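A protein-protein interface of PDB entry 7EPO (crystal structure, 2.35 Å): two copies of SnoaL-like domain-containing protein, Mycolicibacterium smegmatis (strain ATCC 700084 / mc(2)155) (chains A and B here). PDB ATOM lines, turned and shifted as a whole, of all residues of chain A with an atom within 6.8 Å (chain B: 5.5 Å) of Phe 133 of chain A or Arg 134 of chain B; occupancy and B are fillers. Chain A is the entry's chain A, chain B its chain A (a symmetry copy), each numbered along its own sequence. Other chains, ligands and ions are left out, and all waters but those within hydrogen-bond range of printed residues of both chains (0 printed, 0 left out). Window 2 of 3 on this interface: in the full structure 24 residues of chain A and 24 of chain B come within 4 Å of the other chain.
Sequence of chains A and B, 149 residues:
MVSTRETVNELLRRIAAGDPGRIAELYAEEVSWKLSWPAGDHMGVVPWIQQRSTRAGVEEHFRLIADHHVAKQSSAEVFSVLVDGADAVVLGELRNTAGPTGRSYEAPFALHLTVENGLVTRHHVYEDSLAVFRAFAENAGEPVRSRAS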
ATOM      1  N   TRP A  37     -23.313 -25.446   4.347  1.00  0.00           N
ATOM      2  CA  TRP A  37     -22.999 -24.501   3.288  1.00  0.00           C
ATOM      3  C   TRP A  37     -23.721 -24.931   2.021  1.00  0.00           C
ATOM      4  O   TRP A  37     -23.940 -26.125   1.804  1.00  0.00           O
ATOM      5  CB  TRP A  37     -21.492 -24.438   3.014  1.00  0.00           C
ATOM      6  CG  TRP A  37     -20.757 -23.790   4.084  1.00  0.00           C
ATOM      7  CD1 TRP A  37     -20.611 -24.231   5.361  1.00  0.00           C
ATOM      8  CD2 TRP A  37     -20.073 -22.544   4.007  1.00  0.00           C
ATOM      9  NE1 TRP A  37     -19.854 -23.348   6.085  1.00  0.00           N
ATOM     10  CE2 TRP A  37     -19.523 -22.292   5.282  1.00  0.00           C
ATOM     11  CE3 TRP A  37     -19.863 -21.619   2.982  1.00  0.00           C
ATOM     12  CZ2 TRP A  37     -18.768 -21.162   5.557  1.00  0.00           C
ATOM     13  CZ3 TRP A  37     -19.125 -20.486   3.260  1.00  0.00           C
ATOM     14  CH2 TRP A  37     -18.584 -20.268   4.539  1.00  0.00           C
ATOM     15  N   PRO A  38     -24.130 -23.980   1.192  1.00  0.00           N
ATOM     16  CA  PRO A  38     -24.850 -24.334  -0.034  1.00  0.00           C
ATOM     17  C   PRO A  38     -23.997 -25.216  -0.923  1.00  0.00           C
ATOM     18  O   PRO A  38     -22.773 -25.076  -0.972  1.00  0.00           O
ATOM     19  CB  PRO A  38     -25.120 -22.980  -0.699  1.00  0.00           C
ATOM     20  CG  PRO A  38     -24.969 -21.977   0.439  1.00  0.00           C
ATOM     21  CD  PRO A  38     -23.936 -22.531   1.338  1.00  0.00           C
ATOM     22  N   GLY A  40     -23.765 -25.047  -4.123  1.00  0.00           N
ATOM     23  CA  GLY A  40     -23.121 -24.269  -5.176  1.00  0.00           C
ATOM     24  C   GLY A  40     -21.890 -23.499  -4.744  1.00  0.00           C
ATOM     25  O   GLY A  40     -21.136 -23.035  -5.608  1.00  0.00           O
ATOM     26  N   ASP A  41     -21.667 -23.359  -3.440  1.00  0.00           N
ATOM     27  CA  ASP A  41     -20.539 -22.608  -2.914  1.00  0.00           C
ATOM     28  C   ASP A  41     -19.435 -23.506  -2.380  1.00  0.00           C
ATOM     29  O   ASP A  41     -18.534 -23.025  -1.690  1.00  0.00           O
ATOM     30  CB  ASP A  41     -21.018 -21.646  -1.832  1.00  0.00           C
ATOM     31  CG  ASP A  41     -22.118 -20.735  -2.328  1.00  0.00           C
ATOM     32  OD1 ASP A  41     -22.732 -20.052  -1.498  1.00  0.00           O
ATOM     33  OD2 ASP A  41     -22.365 -20.706  -3.559  1.00  0.00           O
ATOM     34  N   VAL A  45     -15.477 -18.939  -2.587  1.00  0.00           N
ATOM     35  CA  VAL A  45     -14.579 -17.937  -2.020  1.00  0.00           C
ATOM     36  C   VAL A  45     -14.054 -18.360  -0.642  1.00  0.00           C
ATOM     37  O   VAL A  45     -12.948 -17.976  -0.254  1.00  0.00           O
ATOM     38  CB  VAL A  45     -15.282 -16.569  -1.969  1.00  0.00           C
ATOM     39  CG1 VAL A  45     -16.394 -16.576  -0.935  1.00  0.00           C
ATOM     40  CG2 VAL A  45     -14.277 -15.460  -1.694  1.00  0.00           C
ATOM     41  N   VAL A  46     -14.829 -19.150   0.101  1.00  0.00           N
ATOM     42  CA  VAL A  46     -14.340 -19.744   1.364  1.00  0.00           C
ATOM     43  C   VAL A  46     -13.753 -21.101   1.024  1.00  0.00           C
ATOM     44  O   VAL A  46     -14.481 -22.031   0.663  1.00  0.00           O
ATOM     45  CB  VAL A  46     -15.488 -19.873   2.382  1.00  0.00           C
ATOM     46  CG1 VAL A  46     -14.966 -20.463   3.684  1.00  0.00           C
ATOM     47  CG2 VAL A  46     -16.115 -18.517   2.630  1.00  0.00           C
ATOM     48  N   ARG A 103     -10.631  -9.412   7.395  1.00  0.00           N
ATOM     49  CA  ARG A 103     -11.823  -9.177   8.201  1.00  0.00           C
ATOM     50  C   ARG A 103     -11.969 -10.256   9.276  1.00  0.00           C
ATOM     51  O   ARG A 103     -11.896 -11.455   8.982  1.00  0.00           O
ATOM     52  CB  ARG A 103     -13.070  -9.148   7.308  1.00  0.00           C
ATOM     53  CG  ARG A 103     -13.066  -8.133   6.159  1.00  0.00           C
ATOM     54  CD  ARG A 103     -14.040  -8.565   5.061  1.00  0.00           C
ATOM     55  NE  ARG A 103     -14.605  -7.455   4.298  1.00  0.00           N
ATOM     56  CZ  ARG A 103     -15.280  -7.605   3.161  1.00  0.00           C
ATOM     57  NH1 ARG A 103     -15.472  -8.822   2.657  1.00  0.00           N
ATOM     58  NH2 ARG A 103     -15.763  -6.540   2.526  1.00  0.00           N
ATOM     59  N   TYR A 105     -14.010 -12.439  12.093  1.00  0.00           N
ATOM     60  CA  TYR A 105     -15.362 -12.984  12.127  1.00  0.00           C
ATOM     61  C   TYR A 105     -15.541 -13.928  13.315  1.00  0.00           C
ATOM     62  O   TYR A 105     -14.585 -14.476  13.870  1.00  0.00           O
ATOM     63  CB  TYR A 105     -15.719 -13.712  10.808  1.00  0.00           C
ATOM     64  CG  TYR A 105     -15.065 -15.067  10.610  1.00  0.00           C
ATOM     65  CD1 TYR A 105     -15.629 -16.214  11.145  1.00  0.00           C
ATOM     66  CD2 TYR A 105     -13.893 -15.197   9.867  1.00  0.00           C
ATOM     67  CE1 TYR A 105     -15.039 -17.453  10.968  1.00  0.00           C
ATOM     68  CE2 TYR A 105     -13.295 -16.431   9.683  1.00  0.00           C
ATOM     69  CZ  TYR A 105     -13.873 -17.556  10.236  1.00  0.00           C
ATOM     70  OH  TYR A 105     -13.290 -18.790  10.065  1.00  0.00           O
ATOM     71  N   ASP A 128     -22.510 -20.775  11.326  1.00  0.00           N
ATOM     72  CA  ASP A 128     -22.950 -19.506  10.740  1.00  0.00           C
ATOM     73  C   ASP A 128     -22.202 -19.282   9.431  1.00  0.00           C
ATOM     74  O   ASP A 128     -21.196 -18.576   9.356  1.00  0.00           O
ATOM     75  CB  ASP A 128     -22.733 -18.343  11.698  1.00  0.00           C
ATOM     76  CG  ASP A 128     -23.364 -17.046  11.190  1.00  0.00           C
ATOM     77  OD1 ASP A 128     -23.789 -17.002  10.015  1.00  0.00           O
ATOM     78  OD2 ASP A 128     -23.438 -16.065  11.956  1.00  0.00           O
ATOM     79  N   SER A 129     -22.731 -19.900   8.379  1.00  0.00           N
ATOM     80  CA  SER A 129     -22.075 -19.889   7.078  1.00  0.00           C
ATOM     81  C   SER A 129     -22.022 -18.478   6.500  1.00  0.00           C
ATOM     82  O   SER A 129     -21.018 -18.091   5.886  1.00  0.00           O
ATOM     83  CB  SER A 129     -22.803 -20.847   6.130  1.00  0.00           C
ATOM     84  OG  SER A 129     -24.191 -20.559   6.034  1.00  0.00           O
ATOM     85  N   LEU A 130     -23.078 -17.692   6.721  1.00  0.00           N
ATOM     86  CA  LEU A 130     -23.130 -16.335   6.195  1.00  0.00           C
ATOM     87  C   LEU A 130     -22.081 -15.427   6.839  1.00  0.00           C
ATOM     88  O   LEU A 130     -21.539 -14.540   6.169  1.00  0.00           O
ATOM     89  CB  LEU A 130     -24.535 -15.769   6.391  1.00  0.00           C
ATOM     90  CG  LEU A 130     -24.698 -14.292   6.078  1.00  0.00           C
ATOM     91  CD1 LEU A 130     -24.658 -14.108   4.563  1.00  0.00           C
ATOM     92  CD2 LEU A 130     -25.989 -13.717   6.659  1.00  0.00           C
ATOM     93  N   ALA A 131     -21.755 -15.635   8.118  1.00  0.00           N
ATOM     94  CA  ALA A 131     -20.759 -14.774   8.751  1.00  0.00           C
ATOM     95  C   ALA A 131     -19.362 -15.071   8.216  1.00  0.00           C
ATOM     96  O   ALA A 131     -18.584 -14.150   7.920  1.00  0.00           O
ATOM     97  CB  ALA A 131     -20.816 -14.925  10.273  1.00  0.00           C
ATOM     98  N   VAL A 132     -19.025 -16.356   8.107  1.00  0.00           N
ATOM     99  CA  VAL A 132     -17.774 -16.761   7.479  1.00  0.00           C
ATOM    100  C   VAL A 132     -17.707 -16.213   6.058  1.00  0.00           C
ATOM    101  O   VAL A 132     -16.707 -15.616   5.637  1.00  0.00           O
ATOM    102  CB  VAL A 132     -17.649 -18.298   7.497  1.00  0.00           C
ATOM    103  CG1 VAL A 132     -16.355 -18.748   6.828  1.00  0.00           C
ATOM    104  CG2 VAL A 132     -17.761 -18.857   8.948  1.00  0.00           C
ATOM    105  N   PHE A 133     -18.794 -16.381   5.311  1.00  0.00           N
ATOM    106  CA  PHE A 133     -18.803 -15.972   3.919  1.00  0.00           C
ATOM    107  C   PHE A 133     -18.522 -14.477   3.780  1.00  0.00           C
ATOM    108  O   PHE A 133     -17.751 -14.062   2.906  1.00  0.00           O
ATOM    109  CB  PHE A 133     -20.140 -16.351   3.283  1.00  0.00           C
ATOM    110  CG  PHE A 133     -20.299 -15.846   1.877  1.00  0.00           C
ATOM    111  CD1 PHE A 133     -19.811 -16.571   0.816  1.00  0.00           C
ATOM    112  CD2 PHE A 133     -20.896 -14.616   1.629  1.00  0.00           C
ATOM    113  CE1 PHE A 133     -19.942 -16.096  -0.488  1.00  0.00           C
ATOM    114  CE2 PHE A 133     -21.034 -14.132   0.335  1.00  0.00           C
ATOM    115  CZ  PHE A 133     -20.555 -14.878  -0.728  1.00  0.00           C
ATOM    116  N   ARG A 134     -19.130 -13.651   4.645  1.00  0.00           N
ATOM    117  CA  ARG A 134     -18.923 -12.204   4.576  1.00  0.00           C
ATOM    118  C   ARG A 134     -17.494 -11.806   4.919  1.00  0.00           C
ATOM    119  O   ARG A 134     -17.048 -10.724   4.532  1.00  0.00           O
ATOM    120  CB  ARG A 134     -19.894 -11.481   5.509  1.00  0.00           C
ATOM    121  CG  ARG A 134     -21.333 -11.622   5.107  1.00  0.00           C
ATOM    122  CD  ARG A 134     -21.904 -10.305   4.661  1.00  0.00           C
ATOM    123  NE  ARG A 134     -23.353 -10.364   4.545  1.00  0.00           N
ATOM    124  CZ  ARG A 134     -24.177 -10.351   5.585  1.00  0.00           C
ATOM    125  NH1 ARG A 134     -23.692 -10.284   6.817  1.00  0.00           N
ATOM    126  NH2 ARG A 134     -25.485 -10.401   5.392  1.00  0.00           N
ATOM    127  N   ALA A 135     -16.776 -12.651   5.653  1.00  0.00           N
ATOM    128  CA  ALA A 135     -15.371 -12.407   5.925  1.00  0.00           C
ATOM    129  C   ALA A 135     -14.474 -12.654   4.715  1.00  0.00           C
ATOM    130  O   ALA A 135     -13.275 -12.381   4.808  1.00  0.00           O
ATOM    131  CB  ALA A 135     -14.926 -13.284   7.098  1.00  0.00           C
ATOM    132  N   PHE A 136     -15.006 -13.137   3.591  1.00  0.00           N
ATOM    133  CA  PHE A 136     -14.154 -13.575   2.481  1.00  0.00           C
ATOM    134  C   PHE A 136     -14.518 -13.014   1.100  1.00  0.00           C
ATOM    135  O   PHE A 136     -15.499 -12.292   0.937  1.00  0.00           O
ATOM    136  CB  PHE A 136     -14.163 -15.098   2.416  1.00  0.00           C
ATOM    137  CG  PHE A 136     -13.297 -15.758   3.457  1.00  0.00           C
ATOM    138  CD1 PHE A 136     -13.824 -16.147   4.676  1.00  0.00           C
ATOM    139  CD2 PHE A 136     -11.957 -16.020   3.206  1.00  0.00           C
ATOM    140  CE1 PHE A 136     -13.029 -16.777   5.636  1.00  0.00           C
ATOM    141  CE2 PHE A 136     -11.154 -16.655   4.165  1.00  0.00           C
ATOM    142  CZ  PHE A 136     -11.697 -17.030   5.375  1.00  0.00           C
ATOM    143  N   ARG B 103     -37.777 -18.027  -4.176  1.00  0.00           N
ATOM    144  CA  ARG B 103     -36.650 -18.938  -4.327  1.00  0.00           C
ATOM    145  C   ARG B 103     -36.713 -20.052  -3.281  1.00  0.00           C
ATOM    146  O   ARG B 103     -36.873 -19.787  -2.084  1.00  0.00           O
ATOM    147  CB  ARG B 103     -35.328 -18.171  -4.204  1.00  0.00           C
ATOM    148  CG  ARG B 103     -35.123 -16.998  -5.171  1.00  0.00           C
ATOM    149  CD  ARG B 103     -34.098 -16.014  -4.608  1.00  0.00           C
ATOM    150  NE  ARG B 103     -33.358 -15.278  -5.630  1.00  0.00           N
ATOM    151  CZ  ARG B 103     -32.596 -14.217  -5.374  1.00  0.00           C
ATOM    152  NH1 ARG B 103     -32.476 -13.769  -4.126  1.00  0.00           N
ATOM    153  NH2 ARG B 103     -31.953 -13.602  -6.363  1.00  0.00           N
ATOM    154  N   SER B 129     -26.907 -20.486   7.363  1.00  0.00           N
ATOM    155  CA  SER B 129     -27.432 -19.127   7.339  1.00  0.00           C
ATOM    156  C   SER B 129     -27.292 -18.507   5.953  1.00  0.00           C
ATOM    157  O   SER B 129     -28.191 -17.788   5.496  1.00  0.00           O
ATOM    158  CB  SER B 129     -26.716 -18.283   8.397  1.00  0.00           C
ATOM    159  OG  SER B 129     -25.303 -18.315   8.245  1.00  0.00           O
ATOM    160  N   LEU B 130     -26.191 -18.808   5.262  1.00  0.00           N
ATOM    161  CA  LEU B 130     -25.957 -18.251   3.937  1.00  0.00           C
ATOM    162  C   LEU B 130     -26.968 -18.763   2.910  1.00  0.00           C
ATOM    163  O   LEU B 130     -27.356 -18.018   2.001  1.00  0.00           O
ATOM    164  CB  LEU B 130     -24.528 -18.567   3.499  1.00  0.00           C
ATOM    165  CG  LEU B 130     -24.192 -18.229   2.057  1.00  0.00           C
ATOM    166  CD1 LEU B 130     -24.072 -16.712   1.928  1.00  0.00           C
ATOM    167  CD2 LEU B 130     -22.913 -18.916   1.585  1.00  0.00           C
ATOM    168  N   ALA B 131     -27.432 -20.009   3.038  1.00  0.00           N
ATOM    169  CA  ALA B 131     -28.394 -20.518   2.063  1.00  0.00           C
ATOM    170  C   ALA B 131     -29.758 -19.858   2.247  1.00  0.00           C
ATOM    171  O   ALA B 131     -30.411 -19.461   1.268  1.00  0.00           O
ATOM    172  CB  ALA B 131     -28.496 -22.042   2.161  1.00  0.00           C
ATOM    173  N   VAL B 132     -30.206 -19.753   3.498  1.00  0.00           N
ATOM    174  CA  VAL B 132     -31.427 -19.018   3.807  1.00  0.00           C
ATOM    175  C   VAL B 132     -31.305 -17.582   3.309  1.00  0.00           C
ATOM    176  O   VAL B 132     -32.198 -17.048   2.636  1.00  0.00           O
ATOM    177  CB  VAL B 132     -31.701 -19.067   5.323  1.00  0.00           C
ATOM    178  CG1 VAL B 132     -32.964 -18.289   5.674  1.00  0.00           C
ATOM    179  CG2 VAL B 132     -31.783 -20.538   5.834  1.00  0.00           C
ATOM    180  N   PHE B 133     -30.174 -16.949   3.607  1.00  0.00           N
ATOM    181  CA  PHE B 133     -29.994 -15.554   3.254  1.00  0.00           C
ATOM    182  C   PHE B 133     -30.114 -15.346   1.745  1.00  0.00           C
ATOM    183  O   PHE B 133     -30.754 -14.389   1.293  1.00  0.00           O
ATOM    184  CB  PHE B 133     -28.645 -15.062   3.781  1.00  0.00           C
ATOM    185  CG  PHE B 133     -28.306 -13.665   3.347  1.00  0.00           C
ATOM    186  CD1 PHE B 133     -28.760 -12.583   4.062  1.00  0.00           C
ATOM    187  CD2 PHE B 133     -27.572 -13.441   2.188  1.00  0.00           C
ATOM    188  CE1 PHE B 133     -28.462 -11.285   3.652  1.00  0.00           C
ATOM    189  CE2 PHE B 133     -27.265 -12.153   1.769  1.00  0.00           C
ATOM    190  CZ  PHE B 133     -27.712 -11.070   2.506  1.00  0.00           C
ATOM    191  N   ARG B 134     -29.512 -16.242   0.947  1.00  0.00           N
ATOM    192  CA  ARG B 134     -29.569 -16.111  -0.509  1.00  0.00           C
ATOM    193  C   ARG B 134     -30.978 -16.302  -1.052  1.00  0.00           C
ATOM    194  O   ARG B 134     -31.277 -15.842  -2.156  1.00  0.00           O
ATOM    195  CB  ARG B 134     -28.624 -17.114  -1.172  1.00  0.00           C
ATOM    196  CG  ARG B 134     -27.174 -16.858  -0.880  1.00  0.00           C
ATOM    197  CD  ARG B 134     -26.438 -16.433  -2.120  1.00  0.00           C
ATOM    198  NE  ARG B 134     -24.997 -16.460  -1.919  1.00  0.00           N
ATOM    199  CZ  ARG B 134     -24.278 -17.575  -1.894  1.00  0.00           C
ATOM    200  NH1 ARG B 134     -24.869 -18.751  -2.053  1.00  0.00           N
ATOM    201  NH2 ARG B 134     -22.968 -17.512  -1.714  1.00  0.00           N
ATOM    202  N   ALA B 135     -31.841 -16.986  -0.307  1.00  0.00           N
ATOM    203  CA  ALA B 135     -33.235 -17.113  -0.693  1.00  0.00           C
ATOM    204  C   ALA B 135     -34.033 -15.828  -0.486  1.00  0.00           C
ATOM    205  O   ALA B 135     -35.204 -15.796  -0.875  1.00  0.00           O
ATOM    206  CB  ALA B 135     -33.872 -18.261   0.093  1.00  0.00           C
ATOM    207  N   PHE B 136     -33.448 -14.776   0.087  1.00  0.00           N
ATOM    208  CA  PHE B 136     -34.230 -13.601   0.485  1.00  0.00           C
ATOM    209  C   PHE B 136     -33.684 -12.247   0.014  1.00  0.00           C
ATOM    210  O   PHE B 136     -32.626 -12.159  -0.607  1.00  0.00           O
ATOM    211  CB  PHE B 136     -34.363 -13.581   2.003  1.00  0.00           C
ATOM    212  CG  PHE B 136     -35.384 -14.551   2.538  1.00  0.00           C
ATOM    213  CD1 PHE B 136     -35.014 -15.826   2.929  1.00  0.00           C
ATOM    214  CD2 PHE B 136     -36.713 -14.178   2.683  1.00  0.00           C
ATOM    215  CE1 PHE B 136     -35.954 -16.721   3.445  1.00  0.00           C
ATOM    216  CE2 PHE B 136     -37.661 -15.072   3.202  1.00  0.00           C
ATOM    217  CZ  PHE B 136     -37.274 -16.339   3.581  1.00  0.00           C
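Among the printed residues, merely in contact across the chains: Pro 38 of chain A with Leu 130 of chain B (3.8 Å), Pro 38 of chain A with Ala 131 of chain B (3.9 Å), Asp 41 of chain A with Leu 130 of chain B (3.3 Å), Leu 130 of chain A with Leu 130 of chain B (3.6 Å), Leu 130 of chain A with Phe 133 of chain B (3.8 Å), Phe 133 of chain A with Leu 130 of chain B (3.8 Å), Phe 133 of chain A with Arg 134 of chain B (3.6 Å) and Arg 134 of chain A with Phe 133 of chain B (3.6 Å).
Of the 9 printed residues of chain B, 5 touch a printed residue of chain A.
Hydrophobic or aromatic side chains of chain B within 4 Å of the printed part of chain A: Leu 130, Ala 131 and Phe 133.
Ser 129 of chain A touches its own counterpart, Ser 129 of chain B.
Ser 129 of chain A touches Leu 130 of chain B, and with the chains exchanged Leu 130 of chain A touches Ser 129 of chain B.
Leu 130 of chain A touches its own counterpart, Leu 130 of chain B.
Phe 133 of chain A touches Arg 134 of chain B, and with the chains exchanged Arg 134 of chain A touches Phe 133 of chain B.
Positions printed for both chains: 103, 129, 130, 131, 132, 133, 134, 135 and 136.
Of the 13 pairs that touch across the chains among the printed residues, 8 have their exchanged pair printed and touching as well.
Trp 37 of chain A touches none of the printed residues of chain B.
Phe 133 of chain A touches two residues of chain B.
Printed residues of chain B within 4 Å of Arg 134 of chain A: Phe 133 (3.6 Å).
Of the printed residues of chain A, Ser 129 of chain B touches Asp 128 (2.7 Å), Ser 129 (3.0 Å) and Leu 130 (2.8 Å).
Printed residues of chain A within 4 Å of Leu 130 of chain B: Pro 38, Asp 41, Ser 129, Leu 130 and Phe 133.
Of the printed residues of chain A, Ala 131 of chain B touches Pro 38.
The nearest printed residue of chain B that does not touch Phe 133 of chain A is Phe 133 of chain B (6.7 Å).
The side-chain carboxylate of Asp 41 of chain A is in salt-bridge range of the guanidinium group of Arg 134 of chain B, at 2.6 Å.
The backbone NH of Leu 130 of chain A sits at hydrogen-bond distance from the side-chain hydroxyl of Ser 129 of chain B (2.8 Å).
The backbone NH (N) of Leu 130 of chain B is in hydrogen-bond range of the side-chain hydroxyl (OG) of Ser 129 of chain A, at 2.8 Å.
The side-chain hydroxyl (OG) of Ser 129 of chain B lies within hydrogen-bond range of the side-chain carboxylate (OD1) of Asp 128 of chain A.
OG of Ser 129 of chain B lies within hydrogen-bond range of N of Ser 129 of chain A (3.0 Å).
O of Arg 134 of chain B sits at hydrogen-bond distance from NH1 of Arg 103 of chain B (3.1 Å).
The backbone carbonyl oxygen (O) of Arg 134 of chain A lies within hydrogen-bond range of the guanidinium group (NH1) of Arg 103 of chain A (3.1 Å).
The backbone NH (N) of Leu 130 of chain A sits close to the side-chain carboxylate (OD1) of Asp 128 of chain A (3.4 Å).
OD1 of Asp 128 of chain A sits at hydrogen-bond distance from N of Ala 131 of chain A, at 3.1 Å.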
